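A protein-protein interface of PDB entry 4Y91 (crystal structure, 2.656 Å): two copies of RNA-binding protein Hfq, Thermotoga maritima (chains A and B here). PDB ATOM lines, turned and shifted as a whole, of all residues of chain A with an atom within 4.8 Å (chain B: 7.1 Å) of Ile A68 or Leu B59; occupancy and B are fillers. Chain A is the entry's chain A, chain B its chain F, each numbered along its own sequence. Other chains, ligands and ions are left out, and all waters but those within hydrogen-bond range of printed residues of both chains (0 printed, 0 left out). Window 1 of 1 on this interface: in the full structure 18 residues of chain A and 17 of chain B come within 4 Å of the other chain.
Printed residues of chain A that touch a printed residue of chain B: Leu A12, Gln A13, Phe A16, Ile A65, Ser A66, Thr A67, Ile A68, Ile A69 and Pro A70. Hydrophobic or aromatic side chains of chain A that line the printed part of chain B: Leu A12, Phe A16, Ile A65, Ile A69 and Pro A70. Printed residues of chain B that touch a printed residue of chain A: Ser B43, Phe B44, Asp B45, Thr B48, Leu B50, Gln B57, Ser B58, Leu B59, Ile B60 and Tyr B61. Along chain B the printed residues that touch a printed residue of chain A span positions 43 to 61. Among the printed residues, 22 pairs touch across the chains. Among the printed residues, no Asp or Glu carboxylate lies within 4 Å of a Lys or Arg side-chain nitrogen of the other chain.
No position is printed for both chains. Of the 22 pairs that touch across the chains among the printed residues, none has its exchanged pair printed and touching as well.
Among the printed residues, merely in contact across the chains: Pro A70 with Gln B57, Thr A67 with Leu B59, Ser A66 with Ile B60, Ile A69 with Gln B57, Leu A12 with Phe B44, Leu A12 with Ser B43, Phe A16 with Leu B59, Ile A69 with Ser B58, Thr A67 with Ser B58, Gln A13 with Thr B48, Ile A65 with Tyr B61, Ile A68 with Ser B58, Leu A12 with Leu B50, Leu A12 with Thr B48, Thr A67 with Ile B60, Leu A12 with Leu B59 and Ile A68 with Gln B57.
Of the printed residues of chain B, Ile A68 touches Gln B57 (3.996 Å), Ser B58 (3.8 Å) and Leu B59 (3.0 Å). Of the printed residues of chain A, Leu B59 touches Leu A12, Phe A16, Thr A67 and Ile A68. Of the printed residues of chain A, Tyr B61 touches Gln A13 (2.7 Å), Ile A65 (3.8 Å) and Ser A66 (3.1 Å). Printed residues of chain A within 4 Å of Leu B50: Leu A12. Of the printed residues of chain B, Gln A13 touches Asp B45 (2.8 Å), Thr B48 (3.7 Å) and Tyr B61 (2.7 Å). Val B49 touches none of the printed residues of chain A. The nearest printed residue of chain A that does not touch Leu B59 is Ser A66 (4.2 Å). The nearest printed residue of chain B that does not touch Thr A67 is Tyr B61 (5.0 Å).
N of Ile A69 lies within hydrogen-bond range of O of Lys A28, 2.8 Å away. OG of Ser A66 sits close to OG1 of Thr A67 (3.1 Å). The backbone NH of Leu B50 lies within hydrogen-bond range of the backbone carbonyl oxygen of Ser B43, at 2.9 Å. The side-chain carboxylate (OD1) of Asp B45 is in hydrogen-bond range of the side-chain hydroxyl (OG1) of Thr B48, at 2.5 Å. N of Val B49 sits at hydrogen-bond distance from O of Ile B60 (2.9 Å). The backbone carbonyl oxygen (O) of Leu B51 is in hydrogen-bond range of the backbone NH (N) of Ser B58, at 2.7 Å.
The backbone NH of Leu A12 lies within hydrogen-bond range of the side-chain carboxylate of Asp B45, at 3.1 Å. N of Gln A13 lies within hydrogen-bond range of OD2 of Asp B45. OH of Tyr B61 is in hydrogen-bond range of OE1 of Gln A13. O of Ser A66 lies within hydrogen-bond range of N of Tyr B61, at 3.1 Å. The backbone NH of Ile A68 is in hydrogen-bond range of the backbone carbonyl oxygen of Leu B59, 3.0 Å away.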
ATOM      1  N   LEU A  12      17.392 -12.472   7.125  1.00  0.00           N
ATOM      2  CA  LEU A  12      17.832 -13.834   7.414  1.00  0.00           C
ATOM      3  C   LEU A  12      18.462 -13.963   8.804  1.00  0.00           C
ATOM      4  O   LEU A  12      18.253 -14.970   9.493  1.00  0.00           O
ATOM      5  CB  LEU A  12      18.821 -14.310   6.346  1.00  0.00           C
ATOM      6  CG  LEU A  12      19.530 -15.646   6.623  1.00  0.00           C
ATOM      7  CD1 LEU A  12      18.588 -16.823   6.921  1.00  0.00           C
ATOM      8  CD2 LEU A  12      20.413 -15.988   5.457  1.00  0.00           C
ATOM      9  N   GLN A  13      19.245 -12.974   9.240  1.00  0.00           N
ATOM     10  CA  GLN A  13      20.075 -13.224  10.413  1.00  0.00           C
ATOM     11  C   GLN A  13      19.241 -13.226  11.685  1.00  0.00           C
ATOM     12  O   GLN A  13      19.361 -14.136  12.521  1.00  0.00           O
ATOM     13  CB  GLN A  13      21.196 -12.201  10.521  1.00  0.00           C
ATOM     14  CG  GLN A  13      21.952 -12.343  11.812  1.00  0.00           C
ATOM     15  CD  GLN A  13      23.025 -11.311  11.948  1.00  0.00           C
ATOM     16  OE1 GLN A  13      23.810 -11.341  12.890  1.00  0.00           O
ATOM     17  NE2 GLN A  13      23.069 -10.380  11.006  1.00  0.00           N
ATOM     18  N   PHE A  16      16.750 -16.231  11.850  1.00  0.00           N
ATOM     19  CA  PHE A  16      17.449 -17.461  12.199  1.00  0.00           C
ATOM     20  C   PHE A  16      17.861 -17.450  13.662  1.00  0.00           C
ATOM     21  O   PHE A  16      17.658 -18.429  14.392  1.00  0.00           O
ATOM     22  CB  PHE A  16      18.664 -17.619  11.295  1.00  0.00           C
ATOM     23  CG  PHE A  16      19.269 -18.992  11.298  1.00  0.00           C
ATOM     24  CD1 PHE A  16      18.811 -19.968  10.430  1.00  0.00           C
ATOM     25  CD2 PHE A  16      20.339 -19.292  12.125  1.00  0.00           C
ATOM     26  CE1 PHE A  16      19.390 -21.239  10.412  1.00  0.00           C
ATOM     27  CE2 PHE A  16      20.920 -20.565  12.110  1.00  0.00           C
ATOM     28  CZ  PHE A  16      20.443 -21.536  11.251  1.00  0.00           C
ATOM     29  N   LEU A  17      18.425 -16.337  14.120  1.00  0.00           N
ATOM     30  CA  LEU A  17      18.825 -16.270  15.522  1.00  0.00           C
ATOM     31  C   LEU A  17      17.616 -16.308  16.445  1.00  0.00           C
ATOM     32  O   LEU A  17      17.653 -16.944  17.505  1.00  0.00           O
ATOM     33  CB  LEU A  17      19.657 -15.011  15.782  1.00  0.00           C
ATOM     34  CG  LEU A  17      21.069 -15.014  15.193  1.00  0.00           C
ATOM     35  CD1 LEU A  17      21.820 -13.753  15.576  1.00  0.00           C
ATOM     36  CD2 LEU A  17      21.820 -16.254  15.629  1.00  0.00           C
ATOM     37  N   LEU A  20      16.391 -19.854  16.739  1.00  0.00           N
ATOM     38  CA  LEU A  20      17.234 -20.568  17.697  1.00  0.00           C
ATOM     39  C   LEU A  20      16.894 -20.176  19.125  1.00  0.00           C
ATOM     40  O   LEU A  20      16.849 -21.034  20.020  1.00  0.00           O
ATOM     41  CB  LEU A  20      18.714 -20.293  17.416  1.00  0.00           C
ATOM     42  CG  LEU A  20      19.236 -20.748  16.051  1.00  0.00           C
ATOM     43  CD1 LEU A  20      20.723 -20.486  15.942  1.00  0.00           C
ATOM     44  CD2 LEU A  20      18.909 -22.212  15.806  1.00  0.00           C
ATOM     45  N   VAL A  27      23.420 -24.597  19.696  1.00  0.00           N
ATOM     46  CA  VAL A  27      24.267 -24.288  18.546  1.00  0.00           C
ATOM     47  C   VAL A  27      25.736 -24.528  18.878  1.00  0.00           C
ATOM     48  O   VAL A  27      26.143 -24.501  20.043  1.00  0.00           O
ATOM     49  CB  VAL A  27      24.062 -22.844  18.093  1.00  0.00           C
ATOM     50  CG1 VAL A  27      22.654 -22.678  17.708  1.00  0.00           C
ATOM     51  CG2 VAL A  27      24.380 -21.896  19.237  1.00  0.00           C
ATOM     52  N   LYS A  28      26.535 -24.799  17.845  1.00  0.00           N
ATOM     53  CA  LYS A  28      27.987 -24.707  17.946  1.00  0.00           C
ATOM     54  C   LYS A  28      28.364 -23.417  17.245  1.00  0.00           C
ATOM     55  O   LYS A  28      27.963 -23.203  16.098  1.00  0.00           O
ATOM     56  CB  LYS A  28      28.714 -25.899  17.322  1.00  0.00           C
ATOM     57  CG  LYS A  28      28.724 -27.172  18.181  1.00  0.00           C
ATOM     58  CD  LYS A  28      29.874 -28.144  17.790  1.00  0.00           C
ATOM     59  CE  LYS A  28      29.459 -29.203  16.740  1.00  0.00           C
ATOM     60  NZ  LYS A  28      30.619 -29.843  16.016  1.00  0.00           N
ATOM     61  N   VAL A  29      29.060 -22.531  17.955  1.00  0.00           N
ATOM     62  CA  VAL A  29      29.454 -21.234  17.420  1.00  0.00           C
ATOM     63  C   VAL A  29      30.932 -21.315  17.129  1.00  0.00           C
ATOM     64  O   VAL A  29      31.720 -21.667  18.014  1.00  0.00           O
ATOM     65  CB  VAL A  29      29.151 -20.091  18.394  1.00  0.00           C
ATOM     66  CG1 VAL A  29      29.697 -18.815  17.851  1.00  0.00           C
ATOM     67  CG2 VAL A  29      27.658 -19.980  18.615  1.00  0.00           C
ATOM     68  N   ILE A  65      32.591 -14.180  15.179  1.00  0.00           N
ATOM     69  CA  ILE A  65      31.927 -15.420  14.802  1.00  0.00           C
ATOM     70  C   ILE A  65      32.193 -15.684  13.330  1.00  0.00           C
ATOM     71  O   ILE A  65      32.054 -14.785  12.493  1.00  0.00           O
ATOM     72  CB  ILE A  65      30.419 -15.340  15.083  1.00  0.00           C
ATOM     73  CG1 ILE A  65      30.194 -14.925  16.546  1.00  0.00           C
ATOM     74  CG2 ILE A  65      29.758 -16.643  14.710  1.00  0.00           C
ATOM     75  CD1 ILE A  65      28.803 -15.218  17.071  1.00  0.00           C
ATOM     76  N   SER A  66      32.607 -16.902  13.000  1.00  0.00           N
ATOM     77  CA  SER A  66      32.601 -17.261  11.590  1.00  0.00           C
ATOM     78  C   SER A  66      31.329 -17.997  11.210  1.00  0.00           C
ATOM     79  O   SER A  66      30.778 -17.754  10.132  1.00  0.00           O
ATOM     80  CB  SER A  66      33.826 -18.109  11.233  1.00  0.00           C
ATOM     81  OG  SER A  66      33.619 -19.461  11.577  1.00  0.00           O
ATOM     82  N   THR A  67      30.825 -18.857  12.092  1.00  0.00           N
ATOM     83  CA  THR A  67      29.687 -19.696  11.758  1.00  0.00           C
ATOM     84  C   THR A  67      28.918 -20.063  13.012  1.00  0.00           C
ATOM     85  O   THR A  67      29.487 -20.238  14.101  1.00  0.00           O
ATOM     86  CB  THR A  67      30.096 -21.009  11.109  1.00  0.00           C
ATOM     87  OG1 THR A  67      31.213 -20.793  10.220  1.00  0.00           O
ATOM     88  CG2 THR A  67      28.912 -21.542  10.332  1.00  0.00           C
ATOM     89  N   ILE A  68      27.621 -20.231  12.822  1.00  0.00           N
ATOM     90  CA  ILE A  68      26.734 -20.815  13.805  1.00  0.00           C
ATOM     91  C   ILE A  68      26.165 -22.084  13.176  1.00  0.00           C
ATOM     92  O   ILE A  68      25.535 -22.023  12.114  1.00  0.00           O
ATOM     93  CB  ILE A  68      25.631 -19.821  14.188  1.00  0.00           C
ATOM     94  CG1 ILE A  68      26.254 -18.602  14.872  1.00  0.00           C
ATOM     95  CG2 ILE A  68      24.576 -20.484  15.051  1.00  0.00           C
ATOM     96  CD1 ILE A  68      25.269 -17.492  15.161  1.00  0.00           C
ATOM     97  N   ILE A  69      26.408 -23.234  13.796  1.00  0.00           N
ATOM     98  CA  ILE A  69      25.800 -24.459  13.276  1.00  0.00           C
ATOM     99  C   ILE A  69      24.799 -25.071  14.247  1.00  0.00           C
ATOM    100  O   ILE A  69      25.194 -25.599  15.299  1.00  0.00           O
ATOM    101  CB  ILE A  69      26.870 -25.481  12.911  1.00  0.00           C
ATOM    102  CG1 ILE A  69      27.912 -24.783  12.062  1.00  0.00           C
ATOM    103  CG2 ILE A  69      26.217 -26.636  12.181  1.00  0.00           C
ATOM    104  CD1 ILE A  69      28.814 -25.709  11.332  1.00  0.00           C
ATOM    105  N   PRO A  70      23.506 -25.033  13.940  1.00  0.00           N
ATOM    106  CA  PRO A  70      22.515 -25.586  14.868  1.00  0.00           C
ATOM    107  C   PRO A  70      22.494 -27.102  14.801  1.00  0.00           C
ATOM    108  O   PRO A  70      22.632 -27.687  13.729  1.00  0.00           O
ATOM    109  CB  PRO A  70      21.193 -24.983  14.374  1.00  0.00           C
ATOM    110  CG  PRO A  70      21.410 -24.771  12.919  1.00  0.00           C
ATOM    111  CD  PRO A  70      22.864 -24.359  12.798  1.00  0.00           C
ATOM    112  N   SER B  43      19.901 -18.914   1.424  1.00  0.00           N
ATOM    113  CA  SER B  43      19.441 -17.554   1.632  1.00  0.00           C
ATOM    114  C   SER B  43      20.656 -16.709   1.967  1.00  0.00           C
ATOM    115  O   SER B  43      21.735 -17.244   2.226  1.00  0.00           O
ATOM    116  CB  SER B  43      18.399 -17.492   2.753  1.00  0.00           C
ATOM    117  OG  SER B  43      17.515 -16.402   2.566  1.00  0.00           O
ATOM    118  N   PHE B  44      20.474 -15.384   1.949  1.00  0.00           N
ATOM    119  CA  PHE B  44      21.510 -14.453   2.377  1.00  0.00           C
ATOM    120  C   PHE B  44      20.861 -13.106   2.666  1.00  0.00           C
ATOM    121  O   PHE B  44      19.784 -12.784   2.150  1.00  0.00           O
ATOM    122  CB  PHE B  44      22.604 -14.290   1.316  1.00  0.00           C
ATOM    123  CG  PHE B  44      22.076 -13.816  -0.022  1.00  0.00           C
ATOM    124  CD1 PHE B  44      21.861 -12.463  -0.269  1.00  0.00           C
ATOM    125  CD2 PHE B  44      21.781 -14.728  -1.018  1.00  0.00           C
ATOM    126  CE1 PHE B  44      21.364 -12.043  -1.481  1.00  0.00           C
ATOM    127  CE2 PHE B  44      21.292 -14.318  -2.227  1.00  0.00           C
ATOM    128  CZ  PHE B  44      21.078 -12.975  -2.463  1.00  0.00           C
ATOM    129  N   ASP B  45      21.548 -12.309   3.475  1.00  0.00           N
ATOM    130  CA  ASP B  45      21.165 -10.923   3.679  1.00  0.00           C
ATOM    131  C   ASP B  45      22.439 -10.082   3.726  1.00  0.00           C
ATOM    132  O   ASP B  45      23.523 -10.522   3.325  1.00  0.00           O
ATOM    133  CB  ASP B  45      20.259 -10.780   4.920  1.00  0.00           C
ATOM    134  CG  ASP B  45      20.966 -11.103   6.257  1.00  0.00           C
ATOM    135  OD1 ASP B  45      22.209 -11.270   6.303  1.00  0.00           O
ATOM    136  OD2 ASP B  45      20.248 -11.163   7.287  1.00  0.00           O
ATOM    137  N   THR B  48      25.033 -12.050   6.258  1.00  0.00           N
ATOM    138  CA  THR B  48      25.078 -13.481   6.515  1.00  0.00           C
ATOM    139  C   THR B  48      24.671 -14.265   5.270  1.00  0.00           C
ATOM    140  O   THR B  48      23.970 -13.758   4.385  1.00  0.00           O
ATOM    141  CB  THR B  48      24.144 -13.848   7.671  1.00  0.00           C
ATOM    142  OG1 THR B  48      22.805 -13.487   7.311  1.00  0.00           O
ATOM    143  CG2 THR B  48      24.517 -13.086   8.929  1.00  0.00           C
ATOM    144  N   VAL B  49      25.106 -15.531   5.218  1.00  0.00           N
ATOM    145  CA  VAL B  49      24.700 -16.460   4.168  1.00  0.00           C
ATOM    146  C   VAL B  49      24.347 -17.766   4.850  1.00  0.00           C
ATOM    147  O   VAL B  49      25.019 -18.170   5.803  1.00  0.00           O
ATOM    148  CB  VAL B  49      25.798 -16.685   3.097  1.00  0.00           C
ATOM    149  CG1 VAL B  49      25.233 -17.423   1.928  1.00  0.00           C
ATOM    150  CG2 VAL B  49      26.369 -15.366   2.621  1.00  0.00           C
ATOM    151  N   LEU B  50      23.266 -18.405   4.388  1.00  0.00           N
ATOM    152  CA  LEU B  50      22.814 -19.688   4.921  1.00  0.00           C
ATOM    153  C   LEU B  50      23.270 -20.790   3.963  1.00  0.00           C
ATOM    154  O   LEU B  50      22.808 -20.872   2.819  1.00  0.00           O
ATOM    155  CB  LEU B  50      21.297 -19.694   5.120  1.00  0.00           C
ATOM    156  CG  LEU B  50      20.676 -21.004   5.636  1.00  0.00           C
ATOM    157  CD1 LEU B  50      21.500 -21.609   6.790  1.00  0.00           C
ATOM    158  CD2 LEU B  50      19.207 -20.812   6.067  1.00  0.00           C
ATOM    159  N   LEU B  51      24.198 -21.615   4.417  1.00  0.00           N
ATOM    160  CA  LEU B  51      24.777 -22.661   3.591  1.00  0.00           C
ATOM    161  C   LEU B  51      24.285 -24.002   4.104  1.00  0.00           C
ATOM    162  O   LEU B  51      24.522 -24.350   5.268  1.00  0.00           O
ATOM    163  CB  LEU B  51      26.301 -22.597   3.628  1.00  0.00           C
ATOM    164  CG  LEU B  51      27.102 -23.390   2.608  1.00  0.00           C
ATOM    165  CD1 LEU B  51      26.966 -22.668   1.272  1.00  0.00           C
ATOM    166  CD2 LEU B  51      28.566 -23.476   3.063  1.00  0.00           C
ATOM    167  N   GLN B  57      23.071 -27.103   8.375  1.00  0.00           N
ATOM    168  CA  GLN B  57      22.859 -25.720   7.971  1.00  0.00           C
ATOM    169  C   GLN B  57      23.888 -24.851   8.668  1.00  0.00           C
ATOM    170  O   GLN B  57      24.127 -25.011   9.865  1.00  0.00           O
ATOM    171  CB  GLN B  57      21.483 -25.210   8.351  1.00  0.00           C
ATOM    172  CG  GLN B  57      20.427 -26.224   8.392  1.00  0.00           C
ATOM    173  CD  GLN B  57      19.157 -25.611   8.903  1.00  0.00           C
ATOM    174  OE1 GLN B  57      18.853 -25.697  10.097  1.00  0.00           O
ATOM    175  NE2 GLN B  57      18.415 -24.951   8.010  1.00  0.00           N
ATOM    176  N   SER B  58      24.488 -23.931   7.930  1.00  0.00           N
ATOM    177  CA  SER B  58      25.485 -23.039   8.492  1.00  0.00           C
ATOM    178  C   SER B  58      25.039 -21.617   8.232  1.00  0.00           C
ATOM    179  O   SER B  58      24.822 -21.235   7.076  1.00  0.00           O
ATOM    180  CB  SER B  58      26.864 -23.293   7.892  1.00  0.00           C
ATOM    181  OG  SER B  58      27.316 -24.599   8.220  1.00  0.00           O
ATOM    182  N   LEU B  59      24.853 -20.853   9.306  1.00  0.00           N
ATOM    183  CA  LEU B  59      24.758 -19.409   9.187  1.00  0.00           C
ATOM    184  C   LEU B  59      26.194 -18.886   9.287  1.00  0.00           C
ATOM    185  O   LEU B  59      26.761 -18.775  10.377  1.00  0.00           O
ATOM    186  CB  LEU B  59      23.826 -18.829  10.245  1.00  0.00           C
ATOM    187  CG  LEU B  59      23.363 -17.389   9.927  1.00  0.00           C
ATOM    188  CD1 LEU B  59      22.423 -17.377   8.755  1.00  0.00           C
ATOM    189  CD2 LEU B  59      22.707 -16.744  11.128  1.00  0.00           C
ATOM    190  N   ILE B  60      26.786 -18.615   8.125  1.00  0.00           N
ATOM    191  CA  ILE B  60      28.117 -18.028   7.982  1.00  0.00           C
ATOM    192  C   ILE B  60      28.010 -16.506   7.936  1.00  0.00           C
ATOM    193  O   ILE B  60      27.180 -15.951   7.196  1.00  0.00           O
ATOM    194  CB  ILE B  60      28.784 -18.543   6.696  1.00  0.00           C
ATOM    195  CG1 ILE B  60      28.791 -20.076   6.682  1.00  0.00           C
ATOM    196  CG2 ILE B  60      30.158 -17.926   6.503  1.00  0.00           C
ATOM    197  CD1 ILE B  60      29.513 -20.653   5.495  1.00  0.00           C
ATOM    198  N   TYR B  61      28.879 -15.822   8.684  1.00  0.00           N
ATOM    199  CA  TYR B  61      28.972 -14.371   8.586  1.00  0.00           C
ATOM    200  C   TYR B  61      29.837 -13.966   7.385  1.00  0.00           C
ATOM    201  O   TYR B  61      30.916 -14.530   7.168  1.00  0.00           O
ATOM    202  CB  TYR B  61      29.524 -13.796   9.894  1.00  0.00           C
ATOM    203  CG  TYR B  61      28.443 -13.639  10.927  1.00  0.00           C
ATOM    204  CD1 TYR B  61      27.636 -12.493  10.966  1.00  0.00           C
ATOM    205  CD2 TYR B  61      28.188 -14.649  11.834  1.00  0.00           C
ATOM    206  CE1 TYR B  61      26.623 -12.371  11.900  1.00  0.00           C
ATOM    207  CE2 TYR B  61      27.196 -14.531  12.771  1.00  0.00           C
ATOM    208  CZ  TYR B  61      26.417 -13.409  12.805  1.00  0.00           C
ATOM    209  OH  TYR B  61      25.420 -13.362  13.750  1.00  0.00           O
